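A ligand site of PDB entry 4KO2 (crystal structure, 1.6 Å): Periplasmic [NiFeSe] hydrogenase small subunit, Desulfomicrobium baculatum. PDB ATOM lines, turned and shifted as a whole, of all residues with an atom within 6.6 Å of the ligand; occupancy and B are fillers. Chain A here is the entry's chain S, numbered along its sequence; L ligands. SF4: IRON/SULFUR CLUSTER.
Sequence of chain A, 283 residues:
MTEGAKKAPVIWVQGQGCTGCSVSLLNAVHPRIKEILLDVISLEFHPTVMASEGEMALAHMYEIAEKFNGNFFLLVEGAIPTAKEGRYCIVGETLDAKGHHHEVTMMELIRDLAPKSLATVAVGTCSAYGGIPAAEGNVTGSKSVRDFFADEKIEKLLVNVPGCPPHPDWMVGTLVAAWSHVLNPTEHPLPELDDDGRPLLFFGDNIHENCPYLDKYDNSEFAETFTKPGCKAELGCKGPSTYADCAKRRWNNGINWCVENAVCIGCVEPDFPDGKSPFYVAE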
ATOM      1  N   ILE A 207     -28.533   2.437  32.837  1.00  0.00           N
ATOM      2  CA  ILE A 207     -27.555   1.367  33.046  1.00  0.00           C
ATOM      3  C   ILE A 207     -26.138   1.907  32.827  1.00  0.00           C
ATOM      4  O   ILE A 207     -25.275   1.773  33.692  1.00  0.00           O
ATOM      5  CB  ILE A 207     -27.819   0.149  32.119  1.00  0.00           C
ATOM      6  CG1 ILE A 207     -29.190  -0.493  32.422  1.00  0.00           C
ATOM      7  CG2 ILE A 207     -26.629  -0.846  32.139  1.00  0.00           C
ATOM      8  CD1 ILE A 207     -29.185  -1.710  33.326  1.00  0.00           C
ATOM      9  N   HIS A 208     -25.926   2.536  31.669  1.00  0.00           N
ATOM     10  CA  HIS A 208     -24.592   3.028  31.273  1.00  0.00           C
ATOM     11  C   HIS A 208     -24.001   4.025  32.293  1.00  0.00           C
ATOM     12  O   HIS A 208     -22.851   3.867  32.721  1.00  0.00           O
ATOM     13  CB  HIS A 208     -24.712   3.584  29.846  1.00  0.00           C
ATOM     14  CG  HIS A 208     -23.474   4.225  29.312  1.00  0.00           C
ATOM     15  ND1 HIS A 208     -22.389   3.504  28.864  1.00  0.00           N
ATOM     16  CD2 HIS A 208     -23.180   5.534  29.085  1.00  0.00           C
ATOM     17  CE1 HIS A 208     -21.462   4.343  28.410  1.00  0.00           C
ATOM     18  NE2 HIS A 208     -21.920   5.574  28.544  1.00  0.00           N
ATOM     19  N   GLU A 209     -24.796   5.007  32.705  1.00  0.00           N
ATOM     20  CA  GLU A 209     -24.345   6.009  33.694  1.00  0.00           C
ATOM     21  C   GLU A 209     -23.907   5.359  35.000  1.00  0.00           C
ATOM     22  O   GLU A 209     -23.052   5.892  35.720  1.00  0.00           O
ATOM     23  CB  GLU A 209     -25.450   7.039  33.957  1.00  0.00           C
ATOM     24  CG  GLU A 209     -25.754   7.941  32.758  1.00  0.00           C
ATOM     25  CD  GLU A 209     -26.925   8.900  32.994  1.00  0.00           C
ATOM     26  OE1 GLU A 209     -27.316   9.140  34.162  1.00  0.00           O
ATOM     27  OE2 GLU A 209     -27.443   9.429  31.993  1.00  0.00           O
ATOM     28  N   CYS A 211     -22.742   2.118  35.184  1.00  0.00           N
ATOM     29  CA  CYS A 211     -22.009   0.913  34.838  1.00  0.00           C
ATOM     30  C   CYS A 211     -20.584   0.908  35.395  1.00  0.00           C
ATOM     31  O   CYS A 211     -19.879   1.919  35.293  1.00  0.00           O
ATOM     32  CB  CYS A 211     -21.946   0.742  33.339  1.00  0.00           C
ATOM     33  SG  CYS A 211     -21.203  -0.820  32.837  1.00  0.00           S
ATOM     34  N   PRO A 212     -20.141  -0.223  35.963  1.00  0.00           N
ATOM     35  CA  PRO A 212     -18.746  -0.281  36.421  1.00  0.00           C
ATOM     36  C   PRO A 212     -17.692  -0.209  35.296  1.00  0.00           C
ATOM     37  O   PRO A 212     -16.507  -0.033  35.585  1.00  0.00           O
ATOM     38  CB  PRO A 212     -18.655  -1.631  37.140  1.00  0.00           C
ATOM     39  CG  PRO A 212     -19.790  -2.436  36.604  1.00  0.00           C
ATOM     40  CD  PRO A 212     -20.889  -1.455  36.284  1.00  0.00           C
ATOM     41  N   TYR A 213     -18.105  -0.383  34.039  1.00  0.00           N
ATOM     42  CA  TYR A 213     -17.185  -0.281  32.896  1.00  0.00           C
ATOM     43  C   TYR A 213     -17.092   1.134  32.353  1.00  0.00           C
ATOM     44  O   TYR A 213     -16.404   1.348  31.351  1.00  0.00           O
ATOM     45  CB  TYR A 213     -17.619  -1.206  31.751  1.00  0.00           C
ATOM     46  CG  TYR A 213     -17.503  -2.688  32.026  1.00  0.00           C
ATOM     47  CD1 TYR A 213     -18.545  -3.377  32.631  1.00  0.00           C
ATOM     48  CD2 TYR A 213     -16.360  -3.404  31.627  1.00  0.00           C
ATOM     49  CE1 TYR A 213     -18.442  -4.756  32.875  1.00  0.00           C
ATOM     50  CE2 TYR A 213     -16.257  -4.784  31.871  1.00  0.00           C
ATOM     51  CZ  TYR A 213     -17.310  -5.454  32.488  1.00  0.00           C
ATOM     52  OH  TYR A 213     -17.215  -6.806  32.740  1.00  0.00           O
ATOM     53  N   LEU A 214     -17.780   2.082  32.973  1.00  0.00           N
ATOM     54  CA  LEU A 214     -17.818   3.435  32.434  1.00  0.00           C
ATOM     55  C   LEU A 214     -16.426   4.073  32.330  1.00  0.00           C
ATOM     56  O   LEU A 214     -16.153   4.779  31.376  1.00  0.00           O
ATOM     57  CB  LEU A 214     -18.786   4.330  33.228  1.00  0.00           C
ATOM     58  CG  LEU A 214     -19.111   5.696  32.606  1.00  0.00           C
ATOM     59  CD1 LEU A 214     -19.829   5.503  31.284  1.00  0.00           C
ATOM     60  CD2 LEU A 214     -19.952   6.535  33.568  1.00  0.00           C
ATOM     61  N   ASP A 215     -15.542   3.794  33.292  1.00  0.00           N
ATOM     62  CA  ASP A 215     -14.148   4.301  33.221  1.00  0.00           C
ATOM     63  C   ASP A 215     -13.441   3.802  31.963  1.00  0.00           C
ATOM     64  O   ASP A 215     -12.713   4.545  31.303  1.00  0.00           O
ATOM     65  CB  ASP A 215     -13.367   3.921  34.496  1.00  0.00           C
ATOM     66  CG  ASP A 215     -13.236   2.390  34.717  1.00  0.00           C
ATOM     67  OD1 ASP A 215     -14.109   1.600  34.259  1.00  0.00           O
ATOM     68  OD2 ASP A 215     -12.248   1.977  35.368  1.00  0.00           O
ATOM     69  N   LYS A 216     -13.670   2.550  31.608  1.00  0.00           N
ATOM     70  CA  LYS A 216     -13.089   1.954  30.407  1.00  0.00           C
ATOM     71  C   LYS A 216     -13.686   2.553  29.141  1.00  0.00           C
ATOM     72  O   LYS A 216     -12.971   2.874  28.201  1.00  0.00           O
ATOM     73  CB  LYS A 216     -13.269   0.439  30.453  1.00  0.00           C
ATOM     74  CG  LYS A 216     -12.313  -0.252  31.413  1.00  0.00           C
ATOM     75  CD  LYS A 216     -12.849  -1.578  31.925  1.00  0.00           C
ATOM     76  CE  LYS A 216     -11.956  -2.148  33.026  1.00  0.00           C
ATOM     77  NZ  LYS A 216     -12.635  -3.267  33.758  1.00  0.00           N
ATOM     78  N   TYR A 217     -15.011   2.719  29.129  1.00  0.00           N
ATOM     79  CA  TYR A 217     -15.687   3.423  28.040  1.00  0.00           C
ATOM     80  C   TYR A 217     -15.073   4.812  27.818  1.00  0.00           C
ATOM     81  O   TYR A 217     -14.779   5.198  26.668  1.00  0.00           O
ATOM     82  CB  TYR A 217     -17.177   3.561  28.367  1.00  0.00           C
ATOM     83  CG  TYR A 217     -17.963   4.363  27.357  1.00  0.00           C
ATOM     84  CD1 TYR A 217     -18.107   5.742  27.495  1.00  0.00           C
ATOM     85  CD2 TYR A 217     -18.589   3.739  26.272  1.00  0.00           C
ATOM     86  CE1 TYR A 217     -18.838   6.492  26.563  1.00  0.00           C
ATOM     87  CE2 TYR A 217     -19.329   4.469  25.338  1.00  0.00           C
ATOM     88  CZ  TYR A 217     -19.442   5.847  25.495  1.00  0.00           C
ATOM     89  OH  TYR A 217     -20.176   6.573  24.582  1.00  0.00           O
ATOM     90  N   PHE A 222     -12.305  -0.789  24.706  1.00  0.00           N
ATOM     91  CA  PHE A 222     -13.416  -1.620  24.314  1.00  0.00           C
ATOM     92  C   PHE A 222     -12.983  -3.067  24.098  1.00  0.00           C
ATOM     93  O   PHE A 222     -11.988  -3.339  23.430  1.00  0.00           O
ATOM     94  CB  PHE A 222     -14.079  -1.083  23.041  1.00  0.00           C
ATOM     95  CG  PHE A 222     -14.602   0.313  23.179  1.00  0.00           C
ATOM     96  CD1 PHE A 222     -15.727   0.564  23.979  1.00  0.00           C
ATOM     97  CD2 PHE A 222     -13.961   1.383  22.549  1.00  0.00           C
ATOM     98  CE1 PHE A 222     -16.226   1.855  24.120  1.00  0.00           C
ATOM     99  CE2 PHE A 222     -14.453   2.677  22.674  1.00  0.00           C
ATOM    100  CZ  PHE A 222     -15.586   2.916  23.470  1.00  0.00           C
ATOM    101  N   GLY A 230     -12.427  -4.766  28.796  1.00  0.00           N
ATOM    102  CA  GLY A 230     -12.948  -3.515  28.250  1.00  0.00           C
ATOM    103  C   GLY A 230     -14.460  -3.382  28.334  1.00  0.00           C
ATOM    104  O   GLY A 230     -15.173  -4.340  28.612  1.00  0.00           O
ATOM    105  N   CYS A 231     -14.921  -2.163  28.078  1.00  0.00           N
ATOM    106  CA  CYS A 231     -16.339  -1.855  27.916  1.00  0.00           C
ATOM    107  C   CYS A 231     -16.940  -2.710  26.772  1.00  0.00           C
ATOM    108  O   CYS A 231     -16.249  -3.041  25.805  1.00  0.00           O
ATOM    109  CB  CYS A 231     -16.492  -0.350  27.643  1.00  0.00           C
ATOM    110  SG  CYS A 231     -18.048   0.138  26.869  1.00  0.00           S
ATOM    111  N   LYS A 232     -18.216  -3.059  26.902  1.00  0.00           N
ATOM    112  CA  LYS A 232     -18.887  -3.969  25.960  1.00  0.00           C
ATOM    113  C   LYS A 232     -19.577  -3.272  24.788  1.00  0.00           C
ATOM    114  O   LYS A 232     -20.287  -3.925  24.010  1.00  0.00           O
ATOM    115  CB  LYS A 232     -19.935  -4.823  26.703  1.00  0.00           C
ATOM    116  CG  LYS A 232     -19.454  -5.492  27.992  1.00  0.00           C
ATOM    117  CD  LYS A 232     -18.245  -6.434  27.743  1.00  0.00           C
ATOM    118  CE  LYS A 232     -17.959  -7.297  28.942  1.00  0.00           C
ATOM    119  NZ  LYS A 232     -18.959  -8.391  29.129  1.00  0.00           N
ATOM    120  N   ALA A 233     -19.371  -1.957  24.652  1.00  0.00           N
ATOM    121  CA  ALA A 233     -20.123  -1.178  23.665  1.00  0.00           C
ATOM    122  C   ALA A 233     -20.012  -1.724  22.237  1.00  0.00           C
ATOM    123  O   ALA A 233     -21.014  -1.811  21.526  1.00  0.00           O
ATOM    124  CB  ALA A 233     -19.672   0.308  23.680  1.00  0.00           C
ATOM    125  N   GLU A 234     -18.782  -2.063  21.811  1.00  0.00           N
ATOM    126  CA  GLU A 234     -18.583  -2.552  20.448  1.00  0.00           C
ATOM    127  C   GLU A 234     -19.166  -3.946  20.213  1.00  0.00           C
ATOM    128  O   GLU A 234     -19.336  -4.356  19.062  1.00  0.00           O
ATOM    129  CB  GLU A 234     -17.087  -2.555  20.072  1.00  0.00           C
ATOM    130  CG  GLU A 234     -16.460  -1.166  19.995  1.00  0.00           C
ATOM    131  CD  GLU A 234     -14.977  -1.214  19.638  1.00  0.00           C
ATOM    132  OE1 GLU A 234     -14.391  -0.127  19.451  1.00  0.00           O
ATOM    133  OE2 GLU A 234     -14.406  -2.314  19.549  1.00  0.00           O
ATOM    134  N   CYS A 237     -23.587  -3.647  23.357  1.00  0.00           N
ATOM    135  CA  CYS A 237     -24.222  -3.247  24.614  1.00  0.00           C
ATOM    136  C   CYS A 237     -25.247  -2.113  24.448  1.00  0.00           C
ATOM    137  O   CYS A 237     -24.913  -1.046  23.901  1.00  0.00           O
ATOM    138  CB  CYS A 237     -23.175  -2.886  25.672  1.00  0.00           C
ATOM    139  SG  CYS A 237     -23.879  -2.657  27.311  1.00  0.00           S
ATOM    140  N   LYS A 238     -26.479  -2.322  24.924  1.00  0.00           N
ATOM    141  CA  LYS A 238     -27.520  -1.296  24.864  1.00  0.00           C
ATOM    142  C   LYS A 238     -27.708  -0.568  26.193  1.00  0.00           C
ATOM    143  O   LYS A 238     -28.684   0.178  26.368  1.00  0.00           O
ATOM    144  CB  LYS A 238     -28.856  -1.889  24.380  1.00  0.00           C
ATOM    145  CG  LYS A 238     -28.766  -2.609  23.031  1.00  0.00           C
ATOM    146  CD  LYS A 238     -28.108  -1.722  21.964  1.00  0.00           C
ATOM    147  CE  LYS A 238     -28.207  -2.327  20.547  1.00  0.00           C
ATOM    148  NZ  LYS A 238     -27.694  -3.728  20.474  1.00  0.00           N
ATOM    149  N   GLY A 239     -26.773  -0.745  27.112  1.00  0.00           N
ATOM    150  CA  GLY A 239     -26.774   0.023  28.367  1.00  0.00           C
ATOM    151  C   GLY A 239     -27.013   1.511  28.213  1.00  0.00           C
ATOM    152  O   GLY A 239     -27.743   2.089  29.021  1.00  0.00           O
ATOM    153  N   PRO A 240     -26.384   2.166  27.187  1.00  0.00           N
ATOM    154  CA  PRO A 240     -26.589   3.599  27.006  1.00  0.00           C
ATOM    155  C   PRO A 240     -28.038   4.042  26.849  1.00  0.00           C
ATOM    156  O   PRO A 240     -28.370   5.162  27.236  1.00  0.00           O
ATOM    157  CB  PRO A 240     -25.754   3.903  25.752  1.00  0.00           C
ATOM    158  CG  PRO A 240     -24.625   2.919  25.836  1.00  0.00           C
ATOM    159  CD  PRO A 240     -25.318   1.651  26.300  1.00  0.00           C
ATOM    160  N   TRP A 257     -24.530 -10.500  36.087  1.00  0.00           N
ATOM    161  CA  TRP A 257     -25.509  -9.693  35.341  1.00  0.00           C
ATOM    162  C   TRP A 257     -25.096  -9.597  33.889  1.00  0.00           C
ATOM    163  O   TRP A 257     -23.973  -9.994  33.522  1.00  0.00           O
ATOM    164  CB  TRP A 257     -25.758  -8.320  35.967  1.00  0.00           C
ATOM    165  CG  TRP A 257     -24.612  -7.321  35.866  1.00  0.00           C
ATOM    166  CD1 TRP A 257     -23.339  -7.476  36.333  1.00  0.00           C
ATOM    167  CD2 TRP A 257     -24.687  -6.001  35.332  1.00  0.00           C
ATOM    168  NE1 TRP A 257     -22.606  -6.336  36.102  1.00  0.00           N
ATOM    169  CE2 TRP A 257     -23.413  -5.416  35.479  1.00  0.00           C
ATOM    170  CE3 TRP A 257     -25.719  -5.257  34.724  1.00  0.00           C
ATOM    171  CZ2 TRP A 257     -23.117  -4.100  35.051  1.00  0.00           C
ATOM    172  CZ3 TRP A 257     -25.441  -3.957  34.298  1.00  0.00           C
ATOM    173  CH2 TRP A 257     -24.135  -3.389  34.456  1.00  0.00           C
ATOM    174  N   VAL A 259     -24.271  -7.360  31.652  1.00  0.00           N
ATOM    175  CA  VAL A 259     -23.154  -6.565  31.166  1.00  0.00           C
ATOM    176  C   VAL A 259     -21.807  -7.187  31.552  1.00  0.00           C
ATOM    177  O   VAL A 259     -20.919  -7.253  30.713  1.00  0.00           O
ATOM    178  CB  VAL A 259     -23.255  -5.109  31.633  1.00  0.00           C
ATOM    179  CG1 VAL A 259     -21.970  -4.327  31.340  1.00  0.00           C
ATOM    180  CG2 VAL A 259     -24.485  -4.427  30.984  1.00  0.00           C
ATOM    181  N   ALA A 262     -21.751 -10.453  29.323  1.00  0.00           N
ATOM    182  CA  ALA A 262     -21.918 -10.325  27.880  1.00  0.00           C
ATOM    183  C   ALA A 262     -22.271  -8.893  27.511  1.00  0.00           C
ATOM    184  O   ALA A 262     -21.415  -8.029  27.565  1.00  0.00           O
ATOM    185  CB  ALA A 262     -22.971 -11.333  27.365  1.00  0.00           C
ATOM    186  N   VAL A 263     -23.528  -8.643  27.151  1.00  0.00           N
ATOM    187  CA  VAL A 263     -24.034  -7.305  26.830  1.00  0.00           C
ATOM    188  C   VAL A 263     -25.438  -7.125  27.402  1.00  0.00           C
ATOM    189  O   VAL A 263     -26.167  -8.107  27.613  1.00  0.00           O
ATOM    190  CB  VAL A 263     -24.114  -7.059  25.298  1.00  0.00           C
ATOM    191  CG1 VAL A 263     -22.707  -6.957  24.652  1.00  0.00           C
ATOM    192  CG2 VAL A 263     -24.947  -8.160  24.597  1.00  0.00           C
ATOM    193  N   CYS A 264     -25.799  -5.863  27.651  1.00  0.00           N
ATOM    194  CA  CYS A 264     -27.204  -5.513  27.901  1.00  0.00           C
ATOM    195  C   CYS A 264     -27.943  -5.521  26.553  1.00  0.00           C
ATOM    196  O   CYS A 264     -27.441  -4.996  25.558  1.00  0.00           O
ATOM    197  CB  CYS A 264     -27.316  -4.122  28.553  1.00  0.00           C
ATOM    198  SG  CYS A 264     -29.031  -3.552  28.830  1.00  0.00           S
HETATM  199 FE1  SF4 L   1     -19.844  -0.016  28.270  1.00  0.00          FE
HETATM  200 FE2  SF4 L   1     -21.214  -0.406  30.586  1.00  0.00          FE
HETATM  201 FE3  SF4 L   1     -21.954   1.475  28.890  1.00  0.00          FE
HETATM  202 FE4  SF4 L   1     -22.369  -1.157  28.223  1.00  0.00          FE
HETATM  203  S1  SF4 L   1     -23.377   0.017  29.919  1.00  0.00           S
HETATM  204  S2  SF4 L   1     -21.606   0.464  26.841  1.00  0.00           S
HETATM  205  S3  SF4 L   1     -20.428  -2.002  29.152  1.00  0.00           S
HETATM  206  S4  SF4 L   1     -19.958   1.407  30.042  1.00  0.00           S
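N of His 208 sits at hydrogen-bond distance from O of Gly 239.
The side-chain sulfur (SG) of Cys 231 lies close to the backbone NH (N) of Ala 233, 3.3 Å away.
The side-chain sulfur of Cys 211 lies close to the backbone NH of Tyr 213 (3.4 Å).
The backbone NH (N) of Cys 237 sits at hydrogen-bond distance from the backbone carbonyl oxygen (O) of Lys 232 (3.4 Å).
SG of Cys 237 sits close to N of Gly 239 (3.5 Å).
The side-chain sulfur (SG) of Cys 237 sits close to the backbone NH (N) of Cys 264 (3.8 Å).
The backbone carbonyl oxygen (O) of Val 259 sits at hydrogen-bond distance from the side-chain amino group (NZ) of Lys 232 (2.8 Å).
The side-chain amino group (NZ) of Lys 232 is in hydrogen-bond range of the backbone carbonyl oxygen (O) of Ala 262, 2.9 Å away.
The backbone carbonyl oxygen (O) of Tyr 213 sits close to a sulfur (S4) of the ligand (3.8 Å).
Residues that only touch the ligand: Tyr 217, Ala 233, Gly 239, Pro 240 and Val 259.
Hydrophobic or aromatic side chains that line the ligand: His 208, Tyr 213, Tyr 217, Ala 233, Pro 240 and Val 259.
Of the 25 residues printed, 12 come within 4 Å of the ligand.
ND1 of His 208 is bound to FE3 of the ligand.
The side-chain sulfur (SG) of Cys 231 binds an iron atom (FE1) of the ligand (2.3 Å).
SG of Cys 211 binds FE2 of the ligand (2.3 Å).
The side-chain sulfur (SG) of Cys 237 is bound to an iron atom (FE4) of the ligand, at 2.3 Å.
The backbone NH of Lys 232 sits close to a sulfur (S3) of the ligand (3.3 Å).
The backbone NH (N) of Leu 214 sits close to a sulfur (S4) of the ligand (3.7 Å).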
